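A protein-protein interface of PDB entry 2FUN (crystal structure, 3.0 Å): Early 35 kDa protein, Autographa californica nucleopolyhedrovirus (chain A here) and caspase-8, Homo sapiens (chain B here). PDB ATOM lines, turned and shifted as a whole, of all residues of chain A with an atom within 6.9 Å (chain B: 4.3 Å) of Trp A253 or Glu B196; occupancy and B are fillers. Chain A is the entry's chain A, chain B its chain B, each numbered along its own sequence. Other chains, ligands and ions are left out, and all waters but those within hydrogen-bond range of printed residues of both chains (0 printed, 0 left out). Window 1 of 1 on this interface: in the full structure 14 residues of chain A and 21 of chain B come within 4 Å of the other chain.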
ATOM      1  N   TYR A  81       7.318  25.120 -16.160  1.00  0.00           N
ATOM      2  CA  TYR A  81       7.068  25.531 -14.781  1.00  0.00           C
ATOM      3  C   TYR A  81       8.147  26.484 -14.295  1.00  0.00           C
ATOM      4  O   TYR A  81       8.475  26.506 -13.112  1.00  0.00           O
ATOM      5  CB  TYR A  81       7.008  24.316 -13.845  1.00  0.00           C
ATOM      6  CG  TYR A  81       5.851  23.375 -14.107  1.00  0.00           C
ATOM      7  CD1 TYR A  81       4.648  23.842 -14.638  1.00  0.00           C
ATOM      8  CD2 TYR A  81       5.942  22.025 -13.796  1.00  0.00           C
ATOM      9  CE1 TYR A  81       3.569  22.983 -14.852  1.00  0.00           C
ATOM     10  CE2 TYR A  81       4.865  21.163 -14.004  1.00  0.00           C
ATOM     11  CZ  TYR A  81       3.691  21.646 -14.530  1.00  0.00           C
ATOM     12  OH  TYR A  81       2.643  20.786 -14.728  1.00  0.00           O
ATOM     13  N   ASP A  83      10.126  29.930 -13.227  1.00  0.00           N
ATOM     14  CA  ASP A  83       9.771  30.988 -12.299  1.00  0.00           C
ATOM     15  C   ASP A  83       9.384  32.258 -13.018  1.00  0.00           C
ATOM     16  O   ASP A  83      10.140  32.776 -13.840  1.00  0.00           O
ATOM     17  CB  ASP A  83      10.938  31.273 -11.359  1.00  0.00           C
ATOM     18  CG  ASP A  83      11.206  30.131 -10.402  1.00  0.00           C
ATOM     19  OD1 ASP A  83      12.287  30.128  -9.772  1.00  0.00           O
ATOM     20  OD2 ASP A  83      10.337  29.248 -10.269  1.00  0.00           O
ATOM     21  N   THR A 249      10.258  16.883 -11.879  1.00  0.00           N
ATOM     22  CA  THR A 249      10.905  17.722 -10.875  1.00  0.00           C
ATOM     23  C   THR A 249      10.251  17.528  -9.518  1.00  0.00           C
ATOM     24  O   THR A 249       9.088  17.132  -9.423  1.00  0.00           O
ATOM     25  CB  THR A 249      10.825  19.210 -11.276  1.00  0.00           C
ATOM     26  OG1 THR A 249      12.049  19.581 -11.908  1.00  0.00           O
ATOM     27  CG2 THR A 249      10.585  20.108 -10.072  1.00  0.00           C
ATOM     28  N   GLU A 250      11.006  17.821  -8.468  1.00  0.00           N
ATOM     29  CA  GLU A 250      10.522  17.673  -7.107  1.00  0.00           C
ATOM     30  C   GLU A 250      10.166  19.006  -6.458  1.00  0.00           C
ATOM     31  O   GLU A 250      10.514  20.073  -6.965  1.00  0.00           O
ATOM     32  CB  GLU A 250      11.577  16.947  -6.269  1.00  0.00           C
ATOM     33  CG  GLU A 250      13.014  17.464  -6.444  1.00  0.00           C
ATOM     34  CD  GLU A 250      13.654  17.071  -7.776  1.00  0.00           C
ATOM     35  OE1 GLU A 250      13.288  17.647  -8.824  1.00  0.00           O
ATOM     36  OE2 GLU A 250      14.533  16.179  -7.775  1.00  0.00           O
ATOM     37  N   SER A 251       9.457  18.932  -5.338  1.00  0.00           N
ATOM     38  CA  SER A 251       9.065  20.124  -4.605  1.00  0.00           C
ATOM     39  C   SER A 251      10.302  20.895  -4.171  1.00  0.00           C
ATOM     40  O   SER A 251      11.427  20.447  -4.356  1.00  0.00           O
ATOM     41  CB  SER A 251       8.263  19.744  -3.364  1.00  0.00           C
ATOM     42  OG  SER A 251       8.056  20.873  -2.533  1.00  0.00           O
ATOM     43  N   SER A 252      10.088  22.067  -3.597  1.00  0.00           N
ATOM     44  CA  SER A 252      11.194  22.873  -3.125  1.00  0.00           C
ATOM     45  C   SER A 252      11.001  23.097  -1.630  1.00  0.00           C
ATOM     46  O   SER A 252      11.889  23.616  -0.951  1.00  0.00           O
ATOM     47  CB  SER A 252      11.239  24.207  -3.863  1.00  0.00           C
ATOM     48  OG  SER A 252      12.347  24.973  -3.430  1.00  0.00           O
ATOM     49  N   TRP A 253       9.831  22.710  -1.125  1.00  0.00           N
ATOM     50  CA  TRP A 253       9.533  22.844   0.299  1.00  0.00           C
ATOM     51  C   TRP A 253       8.773  21.625   0.837  1.00  0.00           C
ATOM     52  O   TRP A 253       9.303  20.508   0.876  1.00  0.00           O
ATOM     53  CB  TRP A 253       8.714  24.114   0.592  1.00  0.00           C
ATOM     54  CG  TRP A 253       8.836  25.210  -0.428  1.00  0.00           C
ATOM     55  CD1 TRP A 253       8.099  25.347  -1.567  1.00  0.00           C
ATOM     56  CD2 TRP A 253       9.760  26.311  -0.414  1.00  0.00           C
ATOM     57  NE1 TRP A 253       8.501  26.464  -2.264  1.00  0.00           N
ATOM     58  CE2 TRP A 253       9.519  27.079  -1.577  1.00  0.00           C
ATOM     59  CE3 TRP A 253      10.766  26.731   0.471  1.00  0.00           C
ATOM     60  CZ2 TRP A 253      10.255  28.235  -1.889  1.00  0.00           C
ATOM     61  CZ3 TRP A 253      11.500  27.886   0.161  1.00  0.00           C
ATOM     62  CH2 TRP A 253      11.236  28.622  -1.005  1.00  0.00           C
ATOM     63  N   GLY A 254       7.525  21.860   1.235  1.00  0.00           N
ATOM     64  CA  GLY A 254       6.677  20.822   1.800  1.00  0.00           C
ATOM     65  C   GLY A 254       6.629  19.437   1.182  1.00  0.00           C
ATOM     66  O   GLY A 254       7.654  18.846   0.842  1.00  0.00           O
ATOM     67  N   LYS A 255       5.410  18.920   1.059  1.00  0.00           N
ATOM     68  CA  LYS A 255       5.154  17.590   0.516  1.00  0.00           C
ATOM     69  C   LYS A 255       6.021  17.183  -0.673  1.00  0.00           C
ATOM     70  O   LYS A 255       6.614  18.025  -1.348  1.00  0.00           O
ATOM     71  CB  LYS A 255       3.672  17.456   0.148  1.00  0.00           C
ATOM     72  CG  LYS A 255       3.143  18.521  -0.799  1.00  0.00           C
ATOM     73  CD  LYS A 255       1.647  18.344  -1.026  1.00  0.00           C
ATOM     74  CE  LYS A 255       1.330  16.974  -1.618  1.00  0.00           C
ATOM     75  NZ  LYS A 255      -0.138  16.727  -1.707  1.00  0.00           N
ATOM     76  N   SER A 256       6.095  15.875  -0.911  1.00  0.00           N
ATOM     77  CA  SER A 256       6.886  15.338  -2.007  1.00  0.00           C
ATOM     78  C   SER A 256       6.059  15.253  -3.273  1.00  0.00           C
ATOM     79  O   SER A 256       5.736  14.163  -3.747  1.00  0.00           O
ATOM     80  CB  SER A 256       7.412  13.948  -1.660  1.00  0.00           C
ATOM     81  OG  SER A 256       8.071  13.378  -2.777  1.00  0.00           O
ATOM     82  N   GLU A 257       5.716  16.412  -3.817  1.00  0.00           N
ATOM     83  CA  GLU A 257       4.931  16.464  -5.035  1.00  0.00           C
ATOM     84  C   GLU A 257       5.862  16.649  -6.226  1.00  0.00           C
ATOM     85  O   GLU A 257       6.684  17.565  -6.242  1.00  0.00           O
ATOM     86  CB  GLU A 257       3.933  17.618  -4.971  1.00  0.00           C
ATOM     87  CG  GLU A 257       2.533  17.230  -5.416  1.00  0.00           C
ATOM     88  CD  GLU A 257       1.993  18.129  -6.510  1.00  0.00           C
ATOM     89  OE1 GLU A 257       1.936  19.360  -6.296  1.00  0.00           O
ATOM     90  OE2 GLU A 257       1.624  17.600  -7.583  1.00  0.00           O
ATOM     91  N   TYR A 259       6.764  17.197 -10.412  1.00  0.00           N
ATOM     92  CA  TYR A 259       6.314  18.163 -11.411  1.00  0.00           C
ATOM     93  C   TYR A 259       6.774  17.791 -12.814  1.00  0.00           C
ATOM     94  O   TYR A 259       7.812  18.250 -13.266  1.00  0.00           O
ATOM     95  CB  TYR A 259       6.836  19.561 -11.051  1.00  0.00           C
ATOM     96  CG  TYR A 259       6.323  20.058  -9.717  1.00  0.00           C
ATOM     97  CD1 TYR A 259       7.200  20.537  -8.746  1.00  0.00           C
ATOM     98  CD2 TYR A 259       4.961  20.006  -9.406  1.00  0.00           C
ATOM     99  CE1 TYR A 259       6.734  20.944  -7.495  1.00  0.00           C
ATOM    100  CE2 TYR A 259       4.485  20.413  -8.157  1.00  0.00           C
ATOM    101  CZ  TYR A 259       5.375  20.879  -7.206  1.00  0.00           C
ATOM    102  OH  TYR A 259       4.917  21.271  -5.966  1.00  0.00           O
ATOM    103  N   LEU B  44      -1.832  28.564  -4.745  1.00  0.00           N
ATOM    104  CA  LEU B  44      -1.065  27.684  -3.872  1.00  0.00           C
ATOM    105  C   LEU B  44      -0.618  28.385  -2.594  1.00  0.00           C
ATOM    106  O   LEU B  44      -0.519  27.764  -1.536  1.00  0.00           O
ATOM    107  CB  LEU B  44       0.152  27.140  -4.621  1.00  0.00           C
ATOM    108  CG  LEU B  44      -0.176  26.099  -5.691  1.00  0.00           C
ATOM    109  CD1 LEU B  44       1.097  25.627  -6.365  1.00  0.00           C
ATOM    110  CD2 LEU B  44      -0.902  24.931  -5.042  1.00  0.00           C
ATOM    111  N   ASN B 193       6.526  31.064  -8.619  1.00  0.00           N
ATOM    112  CA  ASN B 193       6.603  29.864  -9.426  1.00  0.00           C
ATOM    113  C   ASN B 193       5.206  29.281  -9.561  1.00  0.00           C
ATOM    114  O   ASN B 193       4.546  28.985  -8.558  1.00  0.00           O
ATOM    115  CB  ASN B 193       7.527  28.837  -8.782  1.00  0.00           C
ATOM    116  CG  ASN B 193       7.657  27.590  -9.617  1.00  0.00           C
ATOM    117  OD1 ASN B 193       8.291  27.603 -10.671  1.00  0.00           O
ATOM    118  ND2 ASN B 193       7.040  26.507  -9.165  1.00  0.00           N
ATOM    119  N   PRO B 194       4.740  29.102 -10.809  1.00  0.00           N
ATOM    120  CA  PRO B 194       3.413  28.557 -11.127  1.00  0.00           C
ATOM    121  C   PRO B 194       3.112  27.191 -10.520  1.00  0.00           C
ATOM    122  O   PRO B 194       1.993  26.936 -10.096  1.00  0.00           O
ATOM    123  CB  PRO B 194       3.413  28.533 -12.649  1.00  0.00           C
ATOM    124  CG  PRO B 194       4.874  28.309 -12.978  1.00  0.00           C
ATOM    125  CD  PRO B 194       5.548  29.266 -12.032  1.00  0.00           C
ATOM    126  N   ALA B 195       4.117  26.323 -10.465  1.00  0.00           N
ATOM    127  CA  ALA B 195       3.944  24.976  -9.929  1.00  0.00           C
ATOM    128  C   ALA B 195       3.911  24.857  -8.401  1.00  0.00           C
ATOM    129  O   ALA B 195       3.047  24.176  -7.849  1.00  0.00           O
ATOM    130  CB  ALA B 195       5.027  24.064 -10.488  1.00  0.00           C
ATOM    131  N   GLU B 196       4.849  25.505  -7.718  1.00  0.00           N
ATOM    132  CA  GLU B 196       4.917  25.426  -6.260  1.00  0.00           C
ATOM    133  C   GLU B 196       4.273  26.619  -5.557  1.00  0.00           C
ATOM    134  O   GLU B 196       3.461  26.445  -4.652  1.00  0.00           O
ATOM    135  CB  GLU B 196       6.382  25.272  -5.823  1.00  0.00           C
ATOM    136  CG  GLU B 196       7.034  23.990  -6.340  1.00  0.00           C
ATOM    137  CD  GLU B 196       8.546  24.083  -6.480  1.00  0.00           C
ATOM    138  OE1 GLU B 196       9.135  23.225  -7.176  1.00  0.00           O
ATOM    139  OE2 GLU B 196       9.149  25.004  -5.898  1.00  0.00           O
ATOM    140  N   GLY B 197       4.627  27.827  -5.980  1.00  0.00           N
ATOM    141  CA  GLY B 197       4.066  29.019  -5.371  1.00  0.00           C
ATOM    142  C   GLY B 197       5.115  30.102  -5.415  1.00  0.00           C
ATOM    143  O   GLY B 197       5.992  30.059  -6.267  1.00  0.00           O
ATOM    144  N   TRP B 199       8.296  32.254  -3.647  1.00  0.00           N
ATOM    145  CA  TRP B 199       9.368  32.073  -2.685  1.00  0.00           C
ATOM    146  C   TRP B 199       9.034  32.651  -1.318  1.00  0.00           C
ATOM    147  O   TRP B 199       8.844  31.914  -0.346  1.00  0.00           O
ATOM    148  CB  TRP B 199      10.636  32.728  -3.209  1.00  0.00           C
ATOM    149  CG  TRP B 199      10.989  32.317  -4.602  1.00  0.00           C
ATOM    150  CD1 TRP B 199      10.275  31.498  -5.417  1.00  0.00           C
ATOM    151  CD2 TRP B 199      12.149  32.712  -5.344  1.00  0.00           C
ATOM    152  NE1 TRP B 199      10.915  31.353  -6.620  1.00  0.00           N
ATOM    153  CE2 TRP B 199      12.069  32.089  -6.601  1.00  0.00           C
ATOM    154  CE3 TRP B 199      13.247  33.534  -5.066  1.00  0.00           C
ATOM    155  CZ2 TRP B 199      13.044  32.259  -7.581  1.00  0.00           C
ATOM    156  CZ3 TRP B 199      14.217  33.704  -6.042  1.00  0.00           C
ATOM    157  CH2 TRP B 199      14.110  33.069  -7.283  1.00  0.00           C
ATOM    158  N   GLN B 202       5.986  31.182   0.467  1.00  0.00           N
ATOM    159  CA  GLN B 202       6.177  29.760   0.761  1.00  0.00           C
ATOM    160  C   GLN B 202       7.148  29.571   1.915  1.00  0.00           C
ATOM    161  O   GLN B 202       6.925  28.733   2.789  1.00  0.00           O
ATOM    162  CB  GLN B 202       6.684  29.017  -0.475  1.00  0.00           C
ATOM    163  CG  GLN B 202       5.644  28.847  -1.583  1.00  0.00           C
ATOM    164  CD  GLN B 202       4.560  27.838  -1.230  1.00  0.00           C
ATOM    165  OE1 GLN B 202       3.777  28.035  -0.298  1.00  0.00           O
ATOM    166  NE2 GLN B 202       4.513  26.745  -1.980  1.00  0.00           N
ATOM    167  N   SER B 203       8.225  30.351   1.917  1.00  0.00           N
ATOM    168  CA  SER B 203       9.205  30.268   2.987  1.00  0.00           C
ATOM    169  C   SER B 203       8.561  30.814   4.246  1.00  0.00           C
ATOM    170  O   SER B 203       8.722  30.266   5.331  1.00  0.00           O
ATOM    171  CB  SER B 203      10.439  31.094   2.637  1.00  0.00           C
ATOM    172  OG  SER B 203      11.067  30.580   1.479  1.00  0.00           O
ATOM    173  N   GLN B 206       6.584  27.673   5.402  1.00  0.00           N
ATOM    174  CA  GLN B 206       7.422  26.524   5.739  1.00  0.00           C
ATOM    175  C   GLN B 206       8.276  26.840   6.951  1.00  0.00           C
ATOM    176  O   GLN B 206       8.602  25.959   7.741  1.00  0.00           O
ATOM    177  CB  GLN B 206       8.334  26.176   4.565  1.00  0.00           C
ATOM    178  CG  GLN B 206       8.846  24.752   4.580  1.00  0.00           C
ATOM    179  CD  GLN B 206      10.281  24.667   4.134  1.00  0.00           C
ATOM    180  OE1 GLN B 206      10.780  23.591   3.808  1.00  0.00           O
ATOM    181  NE2 GLN B 206      10.966  25.809   4.129  1.00  0.00           N
ATOM    182  N   LYS B 232      17.484  30.820  -2.824  1.00  0.00           N
ATOM    183  CA  LYS B 232      16.671  30.549  -4.008  1.00  0.00           C
ATOM    184  C   LYS B 232      17.268  31.380  -5.123  1.00  0.00           C
ATOM    185  O   LYS B 232      17.488  32.585  -4.965  1.00  0.00           O
ATOM    186  CB  LYS B 232      15.204  30.945  -3.771  1.00  0.00           C
ATOM    187  CG  LYS B 232      14.317  29.813  -3.264  1.00  0.00           C
ATOM    188  CD  LYS B 232      14.038  28.813  -4.372  1.00  0.00           C
ATOM    189  CE  LYS B 232      13.927  27.402  -3.829  1.00  0.00           C
ATOM    190  NZ  LYS B 232      15.232  26.921  -3.287  1.00  0.00           N
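The backbone carbonyl oxygen (O) of Tyr A81 sits close to the side-chain amide oxygen (OD1) of Asn B193 (2.7 Å).
The side-chain carboxylate (OD2) of Asp A83 sits close to the side-chain amide oxygen (OD1) of Asn B193, 2.7 Å away.
NZ of Lys B232 lies close to OG of Ser A252, at 3.5 Å.
The backbone carbonyl oxygen (O) of Glu A250 sits close to the side-chain carboxylate (OE1) of Glu B196, at 3.4 Å.
The backbone carbonyl oxygen of Thr A249 lies within hydrogen-bond range of the backbone NH of Tyr A259, 2.5 Å away.
OG of Ser A251 lies close to O of Lys A255 (3.4 Å).
The side-chain amide nitrogen (ND2) of Asn B193 lies close to the backbone NH (N) of Ala B195 (3.2 Å).
The backbone NH of Glu B196 sits close to the side-chain amide nitrogen of Asn B193, 2.8 Å away.
The side-chain amide nitrogen of Gln B202 is in hydrogen-bond range of the backbone carbonyl oxygen of Glu B196 (2.9 Å).
O of Trp B199 sits at hydrogen-bond distance from OG of Ser B203 (3.2 Å).
Among the printed residues, merely in contact across the chains: Tyr A81 with Pro B194 (3.97 Å), Tyr A81 with Ala B195 (3.8 Å), Asp A83 with Trp B199 (3.1 Å), Ser A251 with Glu B196 (3.98 Å), Ser A252 with Glu B196 (3.0 Å), Trp A253 with Glu B196 (3.97 Å), Trp A253 with Gln B202 (3.6 Å), Trp A253 with Ser B203 (3.0 Å), Trp A253 with Gln B206 (3.8 Å), Tyr A259 with Ala B195 (3.9 Å) and Tyr A259 with Glu B196 (3.3 Å).
Printed residues of chain B within 4 Å of Trp A253: Glu B196 (3.97 Å), Gln B202 (3.6 Å), Ser B203 (3.0 Å) and Gln B206 (3.8 Å).
Glu A257 touches none of the printed residues of chain B.
Of the printed residues of chain B, Tyr A259 touches Ala B195 and Glu B196.
Leu B44 touches none of the printed residues of chain A.
Of the printed residues of chain A, Ala B195 touches Tyr A81 and Tyr A259.
Glu B196 touches five residues of chain A.
Printed residues of chain A within 4 Å of Trp B199: Asp A83 (3.1 Å).
Hydrophobic or aromatic side chains of chain B within 4 Å of the printed part of chain A: Pro B194, Ala B195 and Trp B199.
Along chain B the printed residues that touch a printed residue of chain A span positions 193 to 232.
Printed residues of chain A that touch a printed residue of chain B: Tyr A81, Asp A83, Glu A250, Ser A251, Ser A252, Trp A253 and Tyr A259.
Hydrophobic or aromatic side chains of chain A within 4 Å of the printed part of chain B: Tyr A81, Trp A253 and Tyr A259.
Among the printed residues, 15 pairs touch across the chains.
Among the printed residues, no Asp or Glu carboxylate lies within 4 Å of a Lys or Arg side-chain nitrogen of the other chain.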
